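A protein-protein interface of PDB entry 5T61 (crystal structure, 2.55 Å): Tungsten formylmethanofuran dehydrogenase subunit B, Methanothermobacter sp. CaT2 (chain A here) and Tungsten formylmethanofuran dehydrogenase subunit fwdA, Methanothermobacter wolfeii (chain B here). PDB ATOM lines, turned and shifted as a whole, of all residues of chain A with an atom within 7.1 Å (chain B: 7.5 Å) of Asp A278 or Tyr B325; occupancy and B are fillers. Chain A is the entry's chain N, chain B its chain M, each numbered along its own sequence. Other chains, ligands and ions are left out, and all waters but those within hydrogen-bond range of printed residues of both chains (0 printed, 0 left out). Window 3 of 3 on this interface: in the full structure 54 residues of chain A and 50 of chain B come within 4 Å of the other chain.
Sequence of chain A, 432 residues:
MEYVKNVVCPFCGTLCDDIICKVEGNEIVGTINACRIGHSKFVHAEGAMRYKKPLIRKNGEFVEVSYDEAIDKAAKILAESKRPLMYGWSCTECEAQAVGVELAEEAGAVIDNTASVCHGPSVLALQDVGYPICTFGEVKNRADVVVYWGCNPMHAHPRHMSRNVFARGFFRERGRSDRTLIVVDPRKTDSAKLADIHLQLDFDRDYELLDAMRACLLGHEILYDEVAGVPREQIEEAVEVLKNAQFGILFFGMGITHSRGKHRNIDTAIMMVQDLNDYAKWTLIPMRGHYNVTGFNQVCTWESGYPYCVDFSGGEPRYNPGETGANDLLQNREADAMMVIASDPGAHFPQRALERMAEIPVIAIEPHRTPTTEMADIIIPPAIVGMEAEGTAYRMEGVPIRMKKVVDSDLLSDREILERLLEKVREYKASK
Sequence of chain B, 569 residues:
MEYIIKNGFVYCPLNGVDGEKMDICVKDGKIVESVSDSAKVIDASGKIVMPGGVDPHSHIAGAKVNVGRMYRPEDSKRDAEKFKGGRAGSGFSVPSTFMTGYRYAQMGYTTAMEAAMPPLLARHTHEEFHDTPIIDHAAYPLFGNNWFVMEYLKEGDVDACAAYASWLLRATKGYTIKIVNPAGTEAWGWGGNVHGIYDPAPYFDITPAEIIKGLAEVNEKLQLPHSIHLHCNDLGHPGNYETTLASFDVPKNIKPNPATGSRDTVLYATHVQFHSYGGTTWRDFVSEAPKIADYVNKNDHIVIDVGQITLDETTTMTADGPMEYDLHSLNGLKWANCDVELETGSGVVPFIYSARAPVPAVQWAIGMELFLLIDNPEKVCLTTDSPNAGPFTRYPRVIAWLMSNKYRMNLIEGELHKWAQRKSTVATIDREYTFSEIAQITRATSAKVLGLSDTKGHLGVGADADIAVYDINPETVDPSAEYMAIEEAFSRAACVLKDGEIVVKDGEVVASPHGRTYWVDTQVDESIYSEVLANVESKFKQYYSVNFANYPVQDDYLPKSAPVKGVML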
ATOM      1  N   LEU A 218      -4.340  12.527  -0.513  1.00  0.00           N
ATOM      2  CA  LEU A 218      -5.602  13.200  -0.791  1.00  0.00           C
ATOM      3  C   LEU A 218      -5.687  13.710  -2.225  1.00  0.00           C
ATOM      4  O   LEU A 218      -6.545  14.551  -2.527  1.00  0.00           O
ATOM      5  CB  LEU A 218      -5.819  14.360   0.188  1.00  0.00           C
ATOM      6  CG  LEU A 218      -5.739  14.072   1.689  1.00  0.00           C
ATOM      7  CD1 LEU A 218      -5.748  15.377   2.483  1.00  0.00           C
ATOM      8  CD2 LEU A 218      -6.857  13.140   2.152  1.00  0.00           C
ATOM      9  N   VAL A 273      -2.627   8.381   9.349  1.00  0.00           N
ATOM     10  CA  VAL A 273      -3.246   7.108   9.707  1.00  0.00           C
ATOM     11  C   VAL A 273      -4.762   7.242   9.693  1.00  0.00           C
ATOM     12  O   VAL A 273      -5.476   6.370   9.185  1.00  0.00           O
ATOM     13  CB  VAL A 273      -2.726   6.632  11.075  1.00  0.00           C
ATOM     14  CG1 VAL A 273      -3.607   5.529  11.629  1.00  0.00           C
ATOM     15  CG2 VAL A 273      -1.286   6.159  10.952  1.00  0.00           C
ATOM     16  N   GLN A 274      -5.276   8.345  10.240  1.00  0.00           N
ATOM     17  CA  GLN A 274      -6.712   8.598  10.206  1.00  0.00           C
ATOM     18  C   GLN A 274      -7.227   8.648   8.772  1.00  0.00           C
ATOM     19  O   GLN A 274      -8.183   7.948   8.419  1.00  0.00           O
ATOM     20  CB  GLN A 274      -7.022   9.901  10.946  1.00  0.00           C
ATOM     21  CG  GLN A 274      -6.850   9.801  12.455  1.00  0.00           C
ATOM     22  CD  GLN A 274      -6.975  11.140  13.149  1.00  0.00           C
ATOM     23  OE1 GLN A 274      -6.888  12.193  12.516  1.00  0.00           O
ATOM     24  NE2 GLN A 274      -7.175  11.111  14.460  1.00  0.00           N
ATOM     25  N   ASP A 275      -6.608   9.486   7.930  1.00  0.00           N
ATOM     26  CA  ASP A 275      -7.082   9.660   6.558  1.00  0.00           C
ATOM     27  C   ASP A 275      -6.905   8.404   5.713  1.00  0.00           C
ATOM     28  O   ASP A 275      -7.681   8.181   4.778  1.00  0.00           O
ATOM     29  CB  ASP A 275      -6.373  10.842   5.894  1.00  0.00           C
ATOM     30  CG  ASP A 275      -6.805  12.175   6.467  1.00  0.00           C
ATOM     31  OD1 ASP A 275      -7.734  12.183   7.297  1.00  0.00           O
ATOM     32  OD2 ASP A 275      -6.223  13.212   6.087  1.00  0.00           O
ATOM     33  N   LEU A 276      -5.898   7.576   6.011  1.00  0.00           N
ATOM     34  CA  LEU A 276      -5.726   6.340   5.252  1.00  0.00           C
ATOM     35  C   LEU A 276      -6.935   5.421   5.345  1.00  0.00           C
ATOM     36  O   LEU A 276      -7.136   4.591   4.452  1.00  0.00           O
ATOM     37  CB  LEU A 276      -4.484   5.582   5.725  1.00  0.00           C
ATOM     38  CG  LEU A 276      -3.141   5.992   5.128  1.00  0.00           C
ATOM     39  CD1 LEU A 276      -1.999   5.548   6.029  1.00  0.00           C
ATOM     40  CD2 LEU A 276      -2.998   5.403   3.731  1.00  0.00           C
ATOM     41  N   ASN A 277      -7.752   5.560   6.392  1.00  0.00           N
ATOM     42  CA  ASN A 277      -8.885   4.661   6.604  1.00  0.00           C
ATOM     43  C   ASN A 277     -10.015   4.842   5.600  1.00  0.00           C
ATOM     44  O   ASN A 277     -10.933   4.017   5.588  1.00  0.00           O
ATOM     45  CB  ASN A 277      -9.412   4.828   8.026  1.00  0.00           C
ATOM     46  CG  ASN A 277      -8.548   4.121   9.037  1.00  0.00           C
ATOM     47  OD1 ASN A 277      -8.853   3.003   9.445  1.00  0.00           O
ATOM     48  ND2 ASN A 277      -7.442   4.745   9.416  1.00  0.00           N
ATOM     49  N   ASP A 278      -9.977   5.884   4.768  1.00  0.00           N
ATOM     50  CA  ASP A 278     -10.914   5.983   3.661  1.00  0.00           C
ATOM     51  C   ASP A 278     -10.520   5.076   2.501  1.00  0.00           C
ATOM     52  O   ASP A 278     -11.345   4.816   1.618  1.00  0.00           O
ATOM     53  CB  ASP A 278     -11.005   7.450   3.230  1.00  0.00           C
ATOM     54  CG  ASP A 278     -11.833   8.280   4.205  1.00  0.00           C
ATOM     55  OD1 ASP A 278     -11.276   9.225   4.804  1.00  0.00           O
ATOM     56  OD2 ASP A 278     -12.998   7.922   4.467  1.00  0.00           O
ATOM     57  N   TYR A 279      -9.283   4.576   2.500  1.00  0.00           N
ATOM     58  CA  TYR A 279      -8.788   3.624   1.515  1.00  0.00           C
ATOM     59  C   TYR A 279      -8.449   2.258   2.093  1.00  0.00           C
ATOM     60  O   TYR A 279      -8.566   1.257   1.381  1.00  0.00           O
ATOM     61  CB  TYR A 279      -7.530   4.186   0.832  1.00  0.00           C
ATOM     62  CG  TYR A 279      -7.762   5.495   0.123  1.00  0.00           C
ATOM     63  CD1 TYR A 279      -8.366   5.530  -1.127  1.00  0.00           C
ATOM     64  CD2 TYR A 279      -7.436   6.700   0.729  1.00  0.00           C
ATOM     65  CE1 TYR A 279      -8.591   6.728  -1.776  1.00  0.00           C
ATOM     66  CE2 TYR A 279      -7.666   7.901   0.094  1.00  0.00           C
ATOM     67  CZ  TYR A 279      -8.243   7.910  -1.159  1.00  0.00           C
ATOM     68  OH  TYR A 279      -8.472   9.109  -1.792  1.00  0.00           O
ATOM     69  N   ALA A 280      -8.041   2.183   3.356  1.00  0.00           N
ATOM     70  CA  ALA A 280      -7.601   0.926   3.935  1.00  0.00           C
ATOM     71  C   ALA A 280      -7.610   1.044   5.448  1.00  0.00           C
ATOM     72  O   ALA A 280      -7.344   2.115   5.997  1.00  0.00           O
ATOM     73  CB  ALA A 280      -6.200   0.547   3.449  1.00  0.00           C
ATOM     74  N   LYS A 281      -7.894  -0.070   6.117  1.00  0.00           N
ATOM     75  CA  LYS A 281      -7.895  -0.056   7.573  1.00  0.00           C
ATOM     76  C   LYS A 281      -6.504   0.288   8.075  1.00  0.00           C
ATOM     77  O   LYS A 281      -5.515  -0.332   7.673  1.00  0.00           O
ATOM     78  CB  LYS A 281      -8.323  -1.412   8.120  1.00  0.00           C
ATOM     79  CG  LYS A 281      -9.296  -1.325   9.265  1.00  0.00           C
ATOM     80  CD  LYS A 281      -8.669  -0.886  10.559  1.00  0.00           C
ATOM     81  CE  LYS A 281      -9.757  -0.521  11.543  1.00  0.00           C
ATOM     82  NZ  LYS A 281      -9.680  -1.302  12.801  1.00  0.00           N
ATOM     83  N   TRP B 188     -15.580  -3.676  11.230  1.00  0.00           N
ATOM     84  CA  TRP B 188     -14.730  -2.501  11.342  1.00  0.00           C
ATOM     85  C   TRP B 188     -13.275  -2.877  11.585  1.00  0.00           C
ATOM     86  O   TRP B 188     -12.385  -2.061  11.324  1.00  0.00           O
ATOM     87  CB  TRP B 188     -15.243  -1.589  12.458  1.00  0.00           C
ATOM     88  CG  TRP B 188     -14.375  -0.399  12.716  1.00  0.00           C
ATOM     89  CD1 TRP B 188     -13.709  -0.103  13.869  1.00  0.00           C
ATOM     90  CD2 TRP B 188     -14.070   0.654  11.794  1.00  0.00           C
ATOM     91  NE1 TRP B 188     -13.009   1.071  13.724  1.00  0.00           N
ATOM     92  CE2 TRP B 188     -13.213   1.556  12.458  1.00  0.00           C
ATOM     93  CE3 TRP B 188     -14.439   0.924  10.471  1.00  0.00           C
ATOM     94  CZ2 TRP B 188     -12.722   2.706  11.846  1.00  0.00           C
ATOM     95  CZ3 TRP B 188     -13.948   2.066   9.865  1.00  0.00           C
ATOM     96  CH2 TRP B 188     -13.101   2.943  10.552  1.00  0.00           C
ATOM     97  N   GLY B 191     -12.170  -2.159   8.524  1.00  0.00           N
ATOM     98  CA  GLY B 191     -12.559  -0.848   8.045  1.00  0.00           C
ATOM     99  C   GLY B 191     -13.941  -0.745   7.449  1.00  0.00           C
ATOM    100  O   GLY B 191     -14.252   0.274   6.821  1.00  0.00           O
ATOM    101  N   ASP B 320     -18.925   1.095  19.258  1.00  0.00           N
ATOM    102  CA  ASP B 320     -19.334   1.172  17.854  1.00  0.00           C
ATOM    103  C   ASP B 320     -18.276   1.947  17.064  1.00  0.00           C
ATOM    104  O   ASP B 320     -18.452   3.104  16.676  1.00  0.00           O
ATOM    105  CB  ASP B 320     -20.711   1.818  17.736  1.00  0.00           C
ATOM    106  CG  ASP B 320     -21.418   1.470  16.435  1.00  0.00           C
ATOM    107  OD1 ASP B 320     -20.736   1.182  15.431  1.00  0.00           O
ATOM    108  OD2 ASP B 320     -22.665   1.504  16.417  1.00  0.00           O
ATOM    109  N   GLY B 321     -17.144   1.276  16.854  1.00  0.00           N
ATOM    110  CA  GLY B 321     -16.034   1.807  16.095  1.00  0.00           C
ATOM    111  C   GLY B 321     -16.371   2.422  14.745  1.00  0.00           C
ATOM    112  O   GLY B 321     -16.004   3.568  14.466  1.00  0.00           O
ATOM    113  N   PRO B 322     -17.078   1.687  13.876  1.00  0.00           N
ATOM    114  CA  PRO B 322     -17.344   2.233  12.533  1.00  0.00           C
ATOM    115  C   PRO B 322     -18.197   3.481  12.570  1.00  0.00           C
ATOM    116  O   PRO B 322     -18.030   4.369  11.725  1.00  0.00           O
ATOM    117  CB  PRO B 322     -18.062   1.084  11.813  1.00  0.00           C
ATOM    118  CG  PRO B 322     -18.629   0.249  12.887  1.00  0.00           C
ATOM    119  CD  PRO B 322     -17.717   0.372  14.065  1.00  0.00           C
ATOM    120  N   MET B 323     -19.120   3.562  13.528  1.00  0.00           N
ATOM    121  CA  MET B 323     -19.963   4.742  13.659  1.00  0.00           C
ATOM    122  C   MET B 323     -19.150   5.963  14.073  1.00  0.00           C
ATOM    123  O   MET B 323     -19.367   7.066  13.555  1.00  0.00           O
ATOM    124  CB  MET B 323     -21.074   4.467  14.673  1.00  0.00           C
ATOM    125  CG  MET B 323     -22.222   5.471  14.686  1.00  0.00           C
ATOM    126  SD  MET B 323     -21.858   6.963  15.633  1.00  0.00           S
ATOM    127  CE  MET B 323     -21.397   6.247  17.208  1.00  0.00           C
ATOM    128  N   GLU B 324     -18.209   5.788  15.003  1.00  0.00           N
ATOM    129  CA  GLU B 324     -17.428   6.925  15.485  1.00  0.00           C
ATOM    130  C   GLU B 324     -16.505   7.472  14.409  1.00  0.00           C
ATOM    131  O   GLU B 324     -16.279   8.686  14.335  1.00  0.00           O
ATOM    132  CB  GLU B 324     -16.639   6.527  16.728  1.00  0.00           C
ATOM    133  CG  GLU B 324     -17.530   6.133  17.862  1.00  0.00           C
ATOM    134  CD  GLU B 324     -17.989   7.322  18.679  1.00  0.00           C
ATOM    135  OE1 GLU B 324     -18.848   7.143  19.572  1.00  0.00           O
ATOM    136  OE2 GLU B 324     -17.540   8.449  18.374  1.00  0.00           O
ATOM    137  N   TYR B 325     -15.972   6.598  13.557  1.00  0.00           N
ATOM    138  CA  TYR B 325     -15.202   7.085  12.421  1.00  0.00           C
ATOM    139  C   TYR B 325     -16.079   7.894  11.476  1.00  0.00           C
ATOM    140  O   TYR B 325     -15.640   8.915  10.934  1.00  0.00           O
ATOM    141  CB  TYR B 325     -14.544   5.922  11.688  1.00  0.00           C
ATOM    142  CG  TYR B 325     -13.740   6.376  10.498  1.00  0.00           C
ATOM    143  CD1 TYR B 325     -12.573   7.109  10.666  1.00  0.00           C
ATOM    144  CD2 TYR B 325     -14.150   6.084   9.207  1.00  0.00           C
ATOM    145  CE1 TYR B 325     -11.832   7.534   9.581  1.00  0.00           C
ATOM    146  CE2 TYR B 325     -13.416   6.503   8.113  1.00  0.00           C
ATOM    147  CZ  TYR B 325     -12.259   7.227   8.307  1.00  0.00           C
ATOM    148  OH  TYR B 325     -11.527   7.645   7.220  1.00  0.00           O
ATOM    149  N   ASP B 326     -17.320   7.447  11.255  1.00  0.00           N
ATOM    150  CA  ASP B 326     -18.252   8.226  10.443  1.00  0.00           C
ATOM    151  C   ASP B 326     -18.549   9.576  11.082  1.00  0.00           C
ATOM    152  O   ASP B 326     -18.664  10.588  10.383  1.00  0.00           O
ATOM    153  CB  ASP B 326     -19.553   7.454  10.219  1.00  0.00           C
ATOM    154  CG  ASP B 326     -19.370   6.242   9.336  1.00  0.00           C
ATOM    155  OD1 ASP B 326     -18.413   6.229   8.536  1.00  0.00           O
ATOM    156  OD2 ASP B 326     -20.198   5.311   9.425  1.00  0.00           O
ATOM    157  N   LEU B 327     -18.696   9.608  12.406  1.00  0.00           N
ATOM    158  CA  LEU B 327     -18.967  10.876  13.072  1.00  0.00           C
ATOM    159  C   LEU B 327     -17.775  11.818  12.938  1.00  0.00           C
ATOM    160  O   LEU B 327     -17.946  13.011  12.660  1.00  0.00           O
ATOM    161  CB  LEU B 327     -19.315  10.634  14.541  1.00  0.00           C
ATOM    162  CG  LEU B 327     -19.922  11.802  15.320  1.00  0.00           C
ATOM    163  CD1 LEU B 327     -21.276  12.170  14.730  1.00  0.00           C
ATOM    164  CD2 LEU B 327     -20.062  11.455  16.797  1.00  0.00           C
ATOM    165  N   HIS B 328     -16.561  11.290  13.122  1.00  0.00           N
ATOM    166  CA  HIS B 328     -15.353  12.076  12.881  1.00  0.00           C
ATOM    167  C   HIS B 328     -15.302  12.581  11.443  1.00  0.00           C
ATOM    168  O   HIS B 328     -14.893  13.721  11.194  1.00  0.00           O
ATOM    169  CB  HIS B 328     -14.114  11.244  13.219  1.00  0.00           C
ATOM    170  CG  HIS B 328     -12.885  11.643  12.461  1.00  0.00           C
ATOM    171  ND1 HIS B 328     -12.199  12.812  12.712  1.00  0.00           N
ATOM    172  CD2 HIS B 328     -12.195  11.005  11.485  1.00  0.00           C
ATOM    173  CE1 HIS B 328     -11.155  12.890  11.905  1.00  0.00           C
ATOM    174  NE2 HIS B 328     -11.127  11.804  11.153  1.00  0.00           N
ATOM    175  N   SER B 329     -15.708  11.746  10.483  1.00  0.00           N
ATOM    176  CA  SER B 329     -15.773  12.195   9.096  1.00  0.00           C
ATOM    177  C   SER B 329     -16.717  13.379   8.932  1.00  0.00           C
ATOM    178  O   SER B 329     -16.483  14.245   8.082  1.00  0.00           O
ATOM    179  CB  SER B 329     -16.201  11.047   8.180  1.00  0.00           C
ATOM    180  OG  SER B 329     -15.243  10.003   8.171  1.00  0.00           O
ATOM    181  N   LEU B 330     -17.788  13.437   9.731  1.00  0.00           N
ATOM    182  CA  LEU B 330     -18.762  14.510   9.570  1.00  0.00           C
ATOM    183  C   LEU B 330     -18.270  15.816  10.189  1.00  0.00           C
ATOM    184  O   LEU B 330     -18.228  16.852   9.515  1.00  0.00           O
ATOM    185  CB  LEU B 330     -20.108  14.114  10.188  1.00  0.00           C
ATOM    186  CG  LEU B 330     -21.082  13.242   9.380  1.00  0.00           C
ATOM    187  CD1 LEU B 330     -22.263  12.800  10.260  1.00  0.00           C
ATOM    188  CD2 LEU B 330     -21.548  13.879   8.067  1.00  0.00           C
ATOM    189  N   ASN B 331     -17.894  15.792  11.472  1.00  0.00           N
ATOM    190  CA  ASN B 331     -17.565  17.024  12.185  1.00  0.00           C
ATOM    191  C   ASN B 331     -16.078  17.361  12.170  1.00  0.00           C
ATOM    192  O   ASN B 331     -15.702  18.440  12.640  1.00  0.00           O
ATOM    193  CB  ASN B 331     -18.088  16.969  13.635  1.00  0.00           C
ATOM    194  CG  ASN B 331     -17.310  16.006  14.533  1.00  0.00           C
ATOM    195  OD1 ASN B 331     -16.352  15.357  14.112  1.00  0.00           O
ATOM    196  ND2 ASN B 331     -17.741  15.909  15.786  1.00  0.00           N
ATOM    197  N   TRP B 335     -10.248  12.131  16.786  1.00  0.00           N
ATOM    198  CA  TRP B 335     -10.853  10.804  16.779  1.00  0.00           C
ATOM    199  C   TRP B 335      -9.892   9.771  17.352  1.00  0.00           C
ATOM    200  O   TRP B 335      -8.767   9.629  16.863  1.00  0.00           O
ATOM    201  CB  TRP B 335     -11.269  10.427  15.357  1.00  0.00           C
ATOM    202  CG  TRP B 335     -11.619   8.998  15.187  1.00  0.00           C
ATOM    203  CD1 TRP B 335     -12.570   8.299  15.868  1.00  0.00           C
ATOM    204  CD2 TRP B 335     -11.032   8.081  14.258  1.00  0.00           C
ATOM    205  NE1 TRP B 335     -12.606   6.999  15.427  1.00  0.00           N
ATOM    206  CE2 TRP B 335     -11.672   6.840  14.436  1.00  0.00           C
ATOM    207  CE3 TRP B 335     -10.024   8.189  13.294  1.00  0.00           C
ATOM    208  CZ2 TRP B 335     -11.338   5.714  13.687  1.00  0.00           C
ATOM    209  CZ3 TRP B 335      -9.694   7.070  12.551  1.00  0.00           C
ATOM    210  CH2 TRP B 335     -10.347   5.847  12.755  1.00  0.00           C
ATOM    211  N   ALA B 336     -10.342   9.041  18.371  1.00  0.00           N
ATOM    212  CA  ALA B 336      -9.597   7.927  18.941  1.00  0.00           C
ATOM    213  C   ALA B 336     -10.308   6.610  18.647  1.00  0.00           C
ATOM    214  O   ALA B 336     -11.533   6.563  18.512  1.00  0.00           O
ATOM    215  CB  ALA B 336      -9.417   8.094  20.454  1.00  0.00           C
ATOM    216  N   ASN B 337      -9.523   5.537  18.563  1.00  0.00           N
ATOM    217  CA  ASN B 337     -10.021   4.215  18.206  1.00  0.00           C
ATOM    218  C   ASN B 337      -9.186   3.166  18.930  1.00  0.00           C
ATOM    219  O   ASN B 337      -7.982   3.349  19.126  1.00  0.00           O
ATOM    220  CB  ASN B 337      -9.964   4.008  16.685  1.00  0.00           C
ATOM    221  CG  ASN B 337     -10.465   2.646  16.258  1.00  0.00           C
ATOM    222  OD1 ASN B 337     -11.661   2.444  16.062  1.00  0.00           O
ATOM    223  ND2 ASN B 337      -9.544   1.701  16.096  1.00  0.00           N
ATOM    224  N   SER B 346     -13.698   0.063  19.542  1.00  0.00           N
ATOM    225  CA  SER B 346     -14.191   1.250  20.233  1.00  0.00           C
ATOM    226  C   SER B 346     -13.720   2.507  19.513  1.00  0.00           C
ATOM    227  O   SER B 346     -12.740   2.487  18.763  1.00  0.00           O
ATOM    228  CB  SER B 346     -13.740   1.262  21.700  1.00  0.00           C
ATOM    229  OG  SER B 346     -12.327   1.311  21.799  1.00  0.00           O
ATOM    230  N   GLY B 347     -14.437   3.602  19.757  1.00  0.00           N
ATOM    231  CA  GLY B 347     -14.089   4.893  19.189  1.00  0.00           C
ATOM    232  C   GLY B 347     -14.558   6.025  20.079  1.00  0.00           C
ATOM    233  O   GLY B 347     -15.507   5.878  20.860  1.00  0.00           O
ATOM    234  N   VAL B 348     -13.877   7.167  19.958  1.00  0.00           N
ATOM    235  CA  VAL B 348     -14.146   8.350  20.775  1.00  0.00           C
ATOM    236  C   VAL B 348     -14.029   9.603  19.912  1.00  0.00           C
ATOM    237  O   VAL B 348     -12.996   9.825  19.270  1.00  0.00           O
ATOM    238  CB  VAL B 348     -13.187   8.450  21.981  1.00  0.00           C
ATOM    239  CG1 VAL B 348     -13.581   9.611  22.869  1.00  0.00           C
ATOM    240  CG2 VAL B 348     -13.185   7.160  22.791  1.00  0.00           C
ATOM    241  N   VAL B 349     -15.078  10.428  19.912  1.00  0.00           N
ATOM    242  CA  VAL B 349     -15.141  11.680  19.151  1.00  0.00           C
ATOM    243  C   VAL B 349     -15.905  12.727  19.957  1.00  0.00           C
ATOM    244  O   VAL B 349     -16.968  12.417  20.514  1.00  0.00           O
ATOM    245  CB  VAL B 349     -15.819  11.492  17.779  1.00  0.00           C
ATOM    246  CG1 VAL B 349     -15.678  12.753  16.933  1.00  0.00           C
ATOM    247  CG2 VAL B 349     -15.264  10.292  17.022  1.00  0.00           C
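The side-chain hydroxyl (OH) of Tyr B325 lies within hydrogen-bond range of the side-chain carboxylate (OD1) of Asp A278, 2.9 Å away.
The backbone carbonyl oxygen (O) of Trp B188 lies close to the side-chain amino group (NZ) of Lys A281, 3.2 Å away.
The backbone carbonyl oxygen of Trp B335 lies within hydrogen-bond range of the side-chain amide nitrogen of Gln A274 (3.2 Å).
The backbone carbonyl oxygen (O) of Val A273 sits at hydrogen-bond distance from the side-chain amide nitrogen (ND2) of Asn A277.
The indole nitrogen of Trp B188 sits at hydrogen-bond distance from the side-chain amide oxygen of Asn B337 (3.0 Å).
O of Gln A274 sits close to ND2 of Asn A277 (3.4 Å).
O of Tyr B325 sits at hydrogen-bond distance from OG of Ser B329, at 3.0 Å.
OH of Tyr B325 touches O of Gln A274, at 3.6 Å.
Tyr B325 touches Asn A277 (OH to C, 3.6 Å).
Lys A281 touches Gly B191.
Of chain A, only Gln A274, Asn A277 and Asp A278 come within 4 Å of Tyr B325.
Of the printed residues of chain A, Gly B191 touches Lys A281.
Of the printed residues of chain B, Lys A281 touches Trp B188 (3.1 Å) and Gly B191 (3.1 Å).
The nearest residue of chain A that does not touch Tyr B325 is Asp A275 (4.6 Å).
The nearest printed residue of chain B that does not touch Gln A274 is His B328 (4.4 Å).
Printed residues of chain A that touch a printed residue of chain B: Gln A274, Asn A277, Asp A278 and Lys A281.
Hydrophobic or aromatic side chains of chain B within 4 Å of the printed part of chain A: Tyr B325 and Trp B335.
Along chain B the printed residues that touch a printed residue of chain A span positions 188 to 335.
Among the printed residues, no Asp or Glu carboxylate lies within 4 Å of a Lys or Arg side-chain nitrogen of the other chain.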
